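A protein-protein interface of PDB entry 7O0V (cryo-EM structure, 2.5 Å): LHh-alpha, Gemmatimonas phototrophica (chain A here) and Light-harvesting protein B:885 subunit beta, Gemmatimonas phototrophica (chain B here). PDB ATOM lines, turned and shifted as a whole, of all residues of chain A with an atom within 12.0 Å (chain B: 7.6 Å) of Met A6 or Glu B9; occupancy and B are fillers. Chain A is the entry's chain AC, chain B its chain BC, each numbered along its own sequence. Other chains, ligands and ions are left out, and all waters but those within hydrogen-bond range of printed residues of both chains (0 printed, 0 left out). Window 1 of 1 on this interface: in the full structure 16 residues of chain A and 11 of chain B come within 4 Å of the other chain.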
ATOM      1  N   FME A   1      -5.840   7.571 -29.236  1.00  0.00           N
ATOM      2  CN  FME A   1      -5.404   8.366 -30.270  1.00  0.00           C
ATOM      3  O1  FME A   1      -4.327   8.977 -30.246  1.00  0.00           O
ATOM      4  CA  FME A   1      -5.093   7.368 -28.027  1.00  0.00           C
ATOM      5  CB  FME A   1      -5.878   6.544 -26.984  1.00  0.00           C
ATOM      6  CG  FME A   1      -7.013   7.330 -26.385  1.00  0.00           C
ATOM      7  SD  FME A   1      -8.230   6.171 -25.824  1.00  0.00           S
ATOM      8  CE  FME A   1      -9.219   5.956 -27.255  1.00  0.00           C
ATOM      9  C   FME A   1      -3.761   6.650 -28.239  1.00  0.00           C
ATOM     10  O   FME A   1      -2.834   6.718 -27.436  1.00  0.00           O
ATOM     11  N   HIS A   2      -3.670   5.949 -29.366  1.00  0.00           N
ATOM     12  CA  HIS A   2      -2.534   5.074 -29.649  1.00  0.00           C
ATOM     13  C   HIS A   2      -1.180   5.782 -29.646  1.00  0.00           C
ATOM     14  O   HIS A   2      -0.180   5.217 -29.210  1.00  0.00           O
ATOM     15  CB  HIS A   2      -2.722   4.410 -31.013  1.00  0.00           C
ATOM     16  CG  HIS A   2      -2.638   5.369 -32.159  1.00  0.00           C
ATOM     17  ND1 HIS A   2      -3.613   6.308 -32.420  1.00  0.00           N
ATOM     18  CD2 HIS A   2      -1.669   5.566 -33.083  1.00  0.00           C
ATOM     19  CE1 HIS A   2      -3.261   7.023 -33.473  1.00  0.00           C
ATOM     20  NE2 HIS A   2      -2.086   6.593 -33.895  1.00  0.00           N
ATOM     21  N   ARG A   3      -1.151   7.021 -30.137  1.00  0.00           N
ATOM     22  CA  ARG A   3       0.105   7.752 -30.245  1.00  0.00           C
ATOM     23  C   ARG A   3       0.723   8.117 -28.896  1.00  0.00           C
ATOM     24  O   ARG A   3       1.845   8.634 -28.876  1.00  0.00           O
ATOM     25  CB  ARG A   3      -0.074   8.966 -31.168  1.00  0.00           C
ATOM     26  CG  ARG A   3      -1.313   9.813 -30.977  1.00  0.00           C
ATOM     27  CD  ARG A   3      -1.255  10.999 -31.936  1.00  0.00           C
ATOM     28  NE  ARG A   3      -1.435  10.596 -33.329  1.00  0.00           N
ATOM     29  CZ  ARG A   3      -2.581  10.640 -33.995  1.00  0.00           C
ATOM     30  NH1 ARG A   3      -3.712  10.992 -33.406  1.00  0.00           N
ATOM     31  NH2 ARG A   3      -2.596  10.302 -35.281  1.00  0.00           N
ATOM     32  N   ILE A   4       0.036   7.865 -27.778  1.00  0.00           N
ATOM     33  CA  ILE A   4       0.720   7.863 -26.484  1.00  0.00           C
ATOM     34  C   ILE A   4       1.824   6.812 -26.448  1.00  0.00           C
ATOM     35  O   ILE A   4       2.854   7.009 -25.791  1.00  0.00           O
ATOM     36  CB  ILE A   4      -0.276   7.670 -25.320  1.00  0.00           C
ATOM     37  CG1 ILE A   4       0.368   8.131 -24.011  1.00  0.00           C
ATOM     38  CG2 ILE A   4      -0.714   6.217 -25.191  1.00  0.00           C
ATOM     39  CD1 ILE A   4      -0.617   8.536 -22.947  1.00  0.00           C
ATOM     40  N   TRP A   5       1.640   5.689 -27.145  1.00  0.00           N
ATOM     41  CA  TRP A   5       2.625   4.616 -27.138  1.00  0.00           C
ATOM     42  C   TRP A   5       3.847   4.919 -27.992  1.00  0.00           C
ATOM     43  O   TRP A   5       4.850   4.207 -27.876  1.00  0.00           O
ATOM     44  CB  TRP A   5       1.988   3.309 -27.619  1.00  0.00           C
ATOM     45  CG  TRP A   5       0.722   2.947 -26.906  1.00  0.00           C
ATOM     46  CD1 TRP A   5      -0.510   2.788 -27.464  1.00  0.00           C
ATOM     47  CD2 TRP A   5       0.567   2.675 -25.507  1.00  0.00           C
ATOM     48  NE1 TRP A   5      -1.426   2.448 -26.500  1.00  0.00           N
ATOM     49  CE2 TRP A   5      -0.791   2.370 -25.290  1.00  0.00           C
ATOM     50  CE3 TRP A   5       1.442   2.665 -24.416  1.00  0.00           C
ATOM     51  CZ2 TRP A   5      -1.295   2.059 -24.029  1.00  0.00           C
ATOM     52  CZ3 TRP A   5       0.940   2.356 -23.165  1.00  0.00           C
ATOM     53  CH2 TRP A   5      -0.415   2.057 -22.981  1.00  0.00           C
ATOM     54  N   MET A   6       3.788   5.938 -28.846  1.00  0.00           N
ATOM     55  CA  MET A   6       4.951   6.309 -29.640  1.00  0.00           C
ATOM     56  C   MET A   6       6.107   6.713 -28.733  1.00  0.00           C
ATOM     57  O   MET A   6       5.922   7.409 -27.732  1.00  0.00           O
ATOM     58  CB  MET A   6       4.600   7.443 -30.601  1.00  0.00           C
ATOM     59  CG  MET A   6       3.621   7.034 -31.689  1.00  0.00           C
ATOM     60  SD  MET A   6       3.037   8.419 -32.682  1.00  0.00           S
ATOM     61  CE  MET A   6       4.580   9.033 -33.352  1.00  0.00           C
ATOM     62  N   GLY A   7       7.309   6.268 -29.094  1.00  0.00           N
ATOM     63  CA  GLY A   7       8.493   6.483 -28.293  1.00  0.00           C
ATOM     64  C   GLY A   7       8.614   5.612 -27.060  1.00  0.00           C
ATOM     65  O   GLY A   7       9.591   5.758 -26.317  1.00  0.00           O
ATOM     66  N   THR A   8       7.661   4.719 -26.814  1.00  0.00           N
ATOM     67  CA  THR A   8       7.767   3.718 -25.761  1.00  0.00           C
ATOM     68  C   THR A   8       8.257   2.391 -26.338  1.00  0.00           C
ATOM     69  O   THR A   8       8.313   2.193 -27.553  1.00  0.00           O
ATOM     70  CB  THR A   8       6.426   3.536 -25.042  1.00  0.00           C
ATOM     71  OG1 THR A   8       5.528   2.789 -25.870  1.00  0.00           O
ATOM     72  CG2 THR A   8       5.805   4.885 -24.708  1.00  0.00           C
ATOM     73  N   ASP A   9       8.628   1.477 -25.442  1.00  0.00           N
ATOM     74  CA  ASP A   9       9.049   0.133 -25.819  1.00  0.00           C
ATOM     75  C   ASP A   9       8.012  -0.862 -25.317  1.00  0.00           C
ATOM     76  O   ASP A   9       7.734  -0.891 -24.108  1.00  0.00           O
ATOM     77  CB  ASP A   9      10.434  -0.149 -25.219  1.00  0.00           C
ATOM     78  CG  ASP A   9      10.906  -1.594 -25.388  1.00  0.00           C
ATOM     79  OD1 ASP A   9      10.193  -2.447 -25.949  1.00  0.00           O
ATOM     80  OD2 ASP A   9      12.037  -1.878 -24.939  1.00  0.00           O
ATOM     81  N   PRO A  10       7.413  -1.681 -26.190  1.00  0.00           N
ATOM     82  CA  PRO A  10       6.395  -2.641 -25.725  1.00  0.00           C
ATOM     83  C   PRO A  10       6.869  -3.600 -24.645  1.00  0.00           C
ATOM     84  O   PRO A  10       6.065  -4.000 -23.795  1.00  0.00           O
ATOM     85  CB  PRO A  10       6.007  -3.383 -27.013  1.00  0.00           C
ATOM     86  CG  PRO A  10       7.204  -3.257 -27.892  1.00  0.00           C
ATOM     87  CD  PRO A  10       7.713  -1.864 -27.618  1.00  0.00           C
ATOM     88  N   HIS A  11       8.146  -3.985 -24.646  1.00  0.00           N
ATOM     89  CA  HIS A  11       8.646  -4.894 -23.618  1.00  0.00           C
ATOM     90  C   HIS A  11       8.880  -4.205 -22.279  1.00  0.00           C
ATOM     91  O   HIS A  11       8.814  -4.863 -21.236  1.00  0.00           O
ATOM     92  CB  HIS A  11       9.913  -5.595 -24.109  1.00  0.00           C
ATOM     93  CG  HIS A  11       9.665  -6.557 -25.231  1.00  0.00           C
ATOM     94  ND1 HIS A  11      10.657  -6.990 -26.083  1.00  0.00           N
ATOM     95  CD2 HIS A  11       8.532  -7.187 -25.621  1.00  0.00           C
ATOM     96  CE1 HIS A  11      10.143  -7.836 -26.958  1.00  0.00           C
ATOM     97  NE2 HIS A  11       8.855  -7.973 -26.698  1.00  0.00           N
ATOM     98  N   ILE A  12       9.153  -2.901 -22.270  1.00  0.00           N
ATOM     99  CA  ILE A  12       9.093  -2.156 -21.016  1.00  0.00           C
ATOM    100  C   ILE A  12       7.654  -2.068 -20.523  1.00  0.00           C
ATOM    101  O   ILE A  12       7.362  -2.357 -19.356  1.00  0.00           O
ATOM    102  CB  ILE A  12       9.729  -0.763 -21.173  1.00  0.00           C
ATOM    103  CG1 ILE A  12      11.241  -0.889 -21.375  1.00  0.00           C
ATOM    104  CG2 ILE A  12       9.428   0.103 -19.960  1.00  0.00           C
ATOM    105  CD1 ILE A  12      11.951   0.436 -21.567  1.00  0.00           C
ATOM    106  N   ILE A  13       6.735  -1.661 -21.403  1.00  0.00           N
ATOM    107  CA  ILE A  13       5.342  -1.445 -21.013  1.00  0.00           C
ATOM    108  C   ILE A  13       4.739  -2.713 -20.415  1.00  0.00           C
ATOM    109  O   ILE A  13       4.119  -2.681 -19.345  1.00  0.00           O
ATOM    110  CB  ILE A  13       4.520  -0.952 -22.219  1.00  0.00           C
ATOM    111  CG1 ILE A  13       5.039   0.399 -22.714  1.00  0.00           C
ATOM    112  CG2 ILE A  13       3.043  -0.869 -21.864  1.00  0.00           C
ATOM    113  CD1 ILE A  13       4.937   1.507 -21.692  1.00  0.00           C
ATOM    114  N   GLY B   6      12.370   2.435 -30.540  1.00  0.00           N
ATOM    115  CA  GLY B   6      11.255   3.294 -30.182  1.00  0.00           C
ATOM    116  C   GLY B   6      10.040   3.094 -31.069  1.00  0.00           C
ATOM    117  O   GLY B   6      10.135   3.155 -32.293  1.00  0.00           O
ATOM    118  N   MET B   7       8.896   2.845 -30.435  1.00  0.00           N
ATOM    119  CA  MET B   7       7.680   2.483 -31.155  1.00  0.00           C
ATOM    120  C   MET B   7       7.172   3.638 -32.015  1.00  0.00           C
ATOM    121  O   MET B   7       7.110   4.786 -31.562  1.00  0.00           O
ATOM    122  CB  MET B   7       6.611   2.031 -30.162  1.00  0.00           C
ATOM    123  CG  MET B   7       5.290   1.634 -30.785  1.00  0.00           C
ATOM    124  SD  MET B   7       4.548   0.231 -29.927  1.00  0.00           S
ATOM    125  CE  MET B   7       4.731   0.727 -28.217  1.00  0.00           C
ATOM    126  N   THR B   8       6.814   3.330 -33.260  1.00  0.00           N
ATOM    127  CA  THR B   8       6.341   4.300 -34.238  1.00  0.00           C
ATOM    128  C   THR B   8       4.816   4.259 -34.363  1.00  0.00           C
ATOM    129  O   THR B   8       4.147   3.356 -33.855  1.00  0.00           O
ATOM    130  CB  THR B   8       6.995   4.057 -35.603  1.00  0.00           C
ATOM    131  OG1 THR B   8       6.575   2.788 -36.119  1.00  0.00           O
ATOM    132  CG2 THR B   8       8.512   4.076 -35.481  1.00  0.00           C
ATOM    133  N   GLU B   9       4.276   5.268 -35.054  1.00  0.00           N
ATOM    134  CA  GLU B   9       2.838   5.541 -35.024  1.00  0.00           C
ATOM    135  C   GLU B   9       2.003   4.374 -35.546  1.00  0.00           C
ATOM    136  O   GLU B   9       0.926   4.091 -35.010  1.00  0.00           O
ATOM    137  CB  GLU B   9       2.534   6.805 -35.829  1.00  0.00           C
ATOM    138  CG  GLU B   9       1.147   7.380 -35.579  1.00  0.00           C
ATOM    139  CD  GLU B   9       1.027   8.833 -36.002  1.00  0.00           C
ATOM    140  OE1 GLU B   9       1.734   9.241 -36.948  1.00  0.00           O
ATOM    141  OE2 GLU B   9       0.221   9.566 -35.391  1.00  0.00           O
ATOM    142  N   GLU B  10       2.474   3.683 -36.584  1.00  0.00           N
ATOM    143  CA  GLU B  10       1.709   2.559 -37.117  1.00  0.00           C
ATOM    144  C   GLU B  10       1.821   1.330 -36.224  1.00  0.00           C
ATOM    145  O   GLU B  10       0.855   0.572 -36.080  1.00  0.00           O
ATOM    146  CB  GLU B  10       2.168   2.234 -38.540  1.00  0.00           C
ATOM    147  CG  GLU B  10       1.300   1.215 -39.286  1.00  0.00           C
ATOM    148  CD  GLU B  10      -0.134   1.675 -39.527  1.00  0.00           C
ATOM    149  OE1 GLU B  10      -0.465   2.845 -39.236  1.00  0.00           O
ATOM    150  OE2 GLU B  10      -0.938   0.855 -40.018  1.00  0.00           O
ATOM    151  N   GLU B  11       2.990   1.124 -35.620  1.00  0.00           N
ATOM    152  CA  GLU B  11       3.131   0.100 -34.590  1.00  0.00           C
ATOM    153  C   GLU B  11       2.229   0.394 -33.399  1.00  0.00           C
ATOM    154  O   GLU B  11       1.563  -0.506 -32.873  1.00  0.00           O
ATOM    155  CB  GLU B  11       4.589   0.022 -34.143  1.00  0.00           C
ATOM    156  CG  GLU B  11       5.554  -0.427 -35.223  1.00  0.00           C
ATOM    157  CD  GLU B  11       7.002  -0.274 -34.801  1.00  0.00           C
ATOM    158  OE1 GLU B  11       7.413   0.866 -34.498  1.00  0.00           O
ATOM    159  OE2 GLU B  11       7.729  -1.288 -34.778  1.00  0.00           O
ATOM    160  N   ALA B  12       2.200   1.655 -32.961  1.00  0.00           N
ATOM    161  CA  ALA B  12       1.357   2.065 -31.842  1.00  0.00           C
ATOM    162  C   ALA B  12      -0.121   1.757 -32.072  1.00  0.00           C
ATOM    163  O   ALA B  12      -0.836   1.423 -31.122  1.00  0.00           O
ATOM    164  CB  ALA B  12       1.553   3.555 -31.568  1.00  0.00           C
ATOM    165  N   ARG B  13      -0.605   1.863 -33.314  1.00  0.00           N
ATOM    166  CA  ARG B  13      -1.987   1.467 -33.588  1.00  0.00           C
ATOM    167  C   ARG B  13      -2.212  -0.011 -33.300  1.00  0.00           C
ATOM    168  O   ARG B  13      -3.206  -0.391 -32.670  1.00  0.00           O
ATOM    169  CB  ARG B  13      -2.363   1.778 -35.038  1.00  0.00           C
ATOM    170  CG  ARG B  13      -2.525   3.249 -35.352  1.00  0.00           C
ATOM    171  CD  ARG B  13      -2.979   3.454 -36.787  1.00  0.00           C
ATOM    172  NE  ARG B  13      -3.135   4.868 -37.104  1.00  0.00           N
ATOM    173  CZ  ARG B  13      -2.163   5.652 -37.546  1.00  0.00           C
ATOM    174  NH1 ARG B  13      -0.998   5.157 -37.932  1.00  0.00           N
ATOM    175  NH2 ARG B  13      -2.384   6.958 -37.658  1.00  0.00           N
ATOM    176  N   ARG B  14      -1.296  -0.860 -33.759  1.00  0.00           N
ATOM    177  CA  ARG B  14      -1.453  -2.299 -33.578  1.00  0.00           C
ATOM    178  C   ARG B  14      -1.264  -2.693 -32.116  1.00  0.00           C
ATOM    179  O   ARG B  14      -2.036  -3.494 -31.578  1.00  0.00           O
ATOM    180  CB  ARG B  14      -0.473  -3.029 -34.495  1.00  0.00           C
ATOM    181  CG  ARG B  14      -0.653  -4.531 -34.584  1.00  0.00           C
ATOM    182  CD  ARG B  14       0.154  -5.089 -35.751  1.00  0.00           C
ATOM    183  NE  ARG B  14       1.571  -4.758 -35.655  1.00  0.00           N
ATOM    184  CZ  ARG B  14       2.196  -3.889 -36.439  1.00  0.00           C
ATOM    185  NH1 ARG B  14       1.616  -3.387 -37.516  1.00  0.00           N
ATOM    186  NH2 ARG B  14       3.454  -3.557 -36.164  1.00  0.00           N
ATOM    187  N   PHE B  15      -0.239  -2.138 -31.465  1.00  0.00           N
ATOM    188  CA  PHE B  15      -0.066  -2.298 -30.022  1.00  0.00           C
ATOM    189  C   PHE B  15      -1.317  -1.885 -29.251  1.00  0.00           C
ATOM    190  O   PHE B  15      -1.843  -2.654 -28.439  1.00  0.00           O
ATOM    191  CB  PHE B  15       1.144  -1.482 -29.559  1.00  0.00           C
ATOM    192  CG  PHE B  15       1.453  -1.630 -28.097  1.00  0.00           C
ATOM    193  CD1 PHE B  15       2.249  -2.669 -27.647  1.00  0.00           C
ATOM    194  CD2 PHE B  15       0.951  -0.730 -27.172  1.00  0.00           C
ATOM    195  CE1 PHE B  15       2.537  -2.809 -26.304  1.00  0.00           C
ATOM    196  CE2 PHE B  15       1.233  -0.866 -25.826  1.00  0.00           C
ATOM    197  CZ  PHE B  15       2.029  -1.907 -25.393  1.00  0.00           C
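Glu B9 touches His A2 (O to CD2, 3.6 Å). Ala B12 touches His A2. Arg B13 touches His A2 (CG to CD2, 3.4 Å). CE of Met B7 touches O of Trp A5, 3.5 Å away. Trp A5 touches Ala B12. Phe B15 touches Trp A5 (CE2 to CD2, 3.6 Å). Met A6 touches Met B7 (CA to O, 3.3 Å). Glu B9 touches Met A6. Phe B15 touches Pro A10. Phe B15 touches Ile A13 (CZ to CG2, 3.8 Å).
Of the printed residues of chain B, Arg A3 touches Glu B9 (2.8 Å). Met A6 touches just these residues of chain B: Met B7 and Glu B9. Of the printed residues of chain B, Ile A13 touches Phe B15 (3.8 Å). No residue of chain A comes within 4 Å of Thr B8. Of the printed residues of chain A, Glu B9 touches His A2, Arg A3 and Met A6. No residue of chain A comes within 4 Å of Glu B10. Glu B11 touches none of the printed residues of chain A. Ala B12 touches just these residues of chain A: His A2 and Trp A5. Arg B13 touches one residue of chain A. The nearest printed residue of chain B that does not touch Met A6 is Thr B8 (4.03 Å). The nearest printed residue of chain B that does not touch Trp A5 is Thr B8 (5.8 Å).
The side-chain hydroxyl of Thr A8 is in hydrogen-bond range of the backbone carbonyl oxygen of Trp A5, 2.5 Å away. NH1 of Arg B13 lies within salt-bridge range of OE1 of Glu B10, 2.7 Å away.
Printed residues of chain B that touch a printed residue of chain A: Met B7, Glu B9, Ala B12, Arg B13 and Phe B15. Along chain B the printed residues that touch a printed residue of chain A span positions 7 to 15. Of the 13 printed residues of chain A, 8 touch a printed residue of chain B. Hydrophobic or aromatic side chains of chain A that line the printed part of chain B: His A2, Trp A5, Met A6, Pro A10 and Ile A13. Among the printed residues, Asp or Glu carboxylates within 4 Å of a Lys or Arg side-chain nitrogen of the other chain: Arg A3 with Glu B9 (2.8 Å).
NE of Arg A3 is in salt-bridge range of OE2 of Glu B9 (2.8 Å). O of Met B7 sits at hydrogen-bond distance from N of Gly A7, 2.9 Å away. The backbone carbonyl oxygen (O) of Thr A8 lies within hydrogen-bond range of the backbone NH (N) of Met B7.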
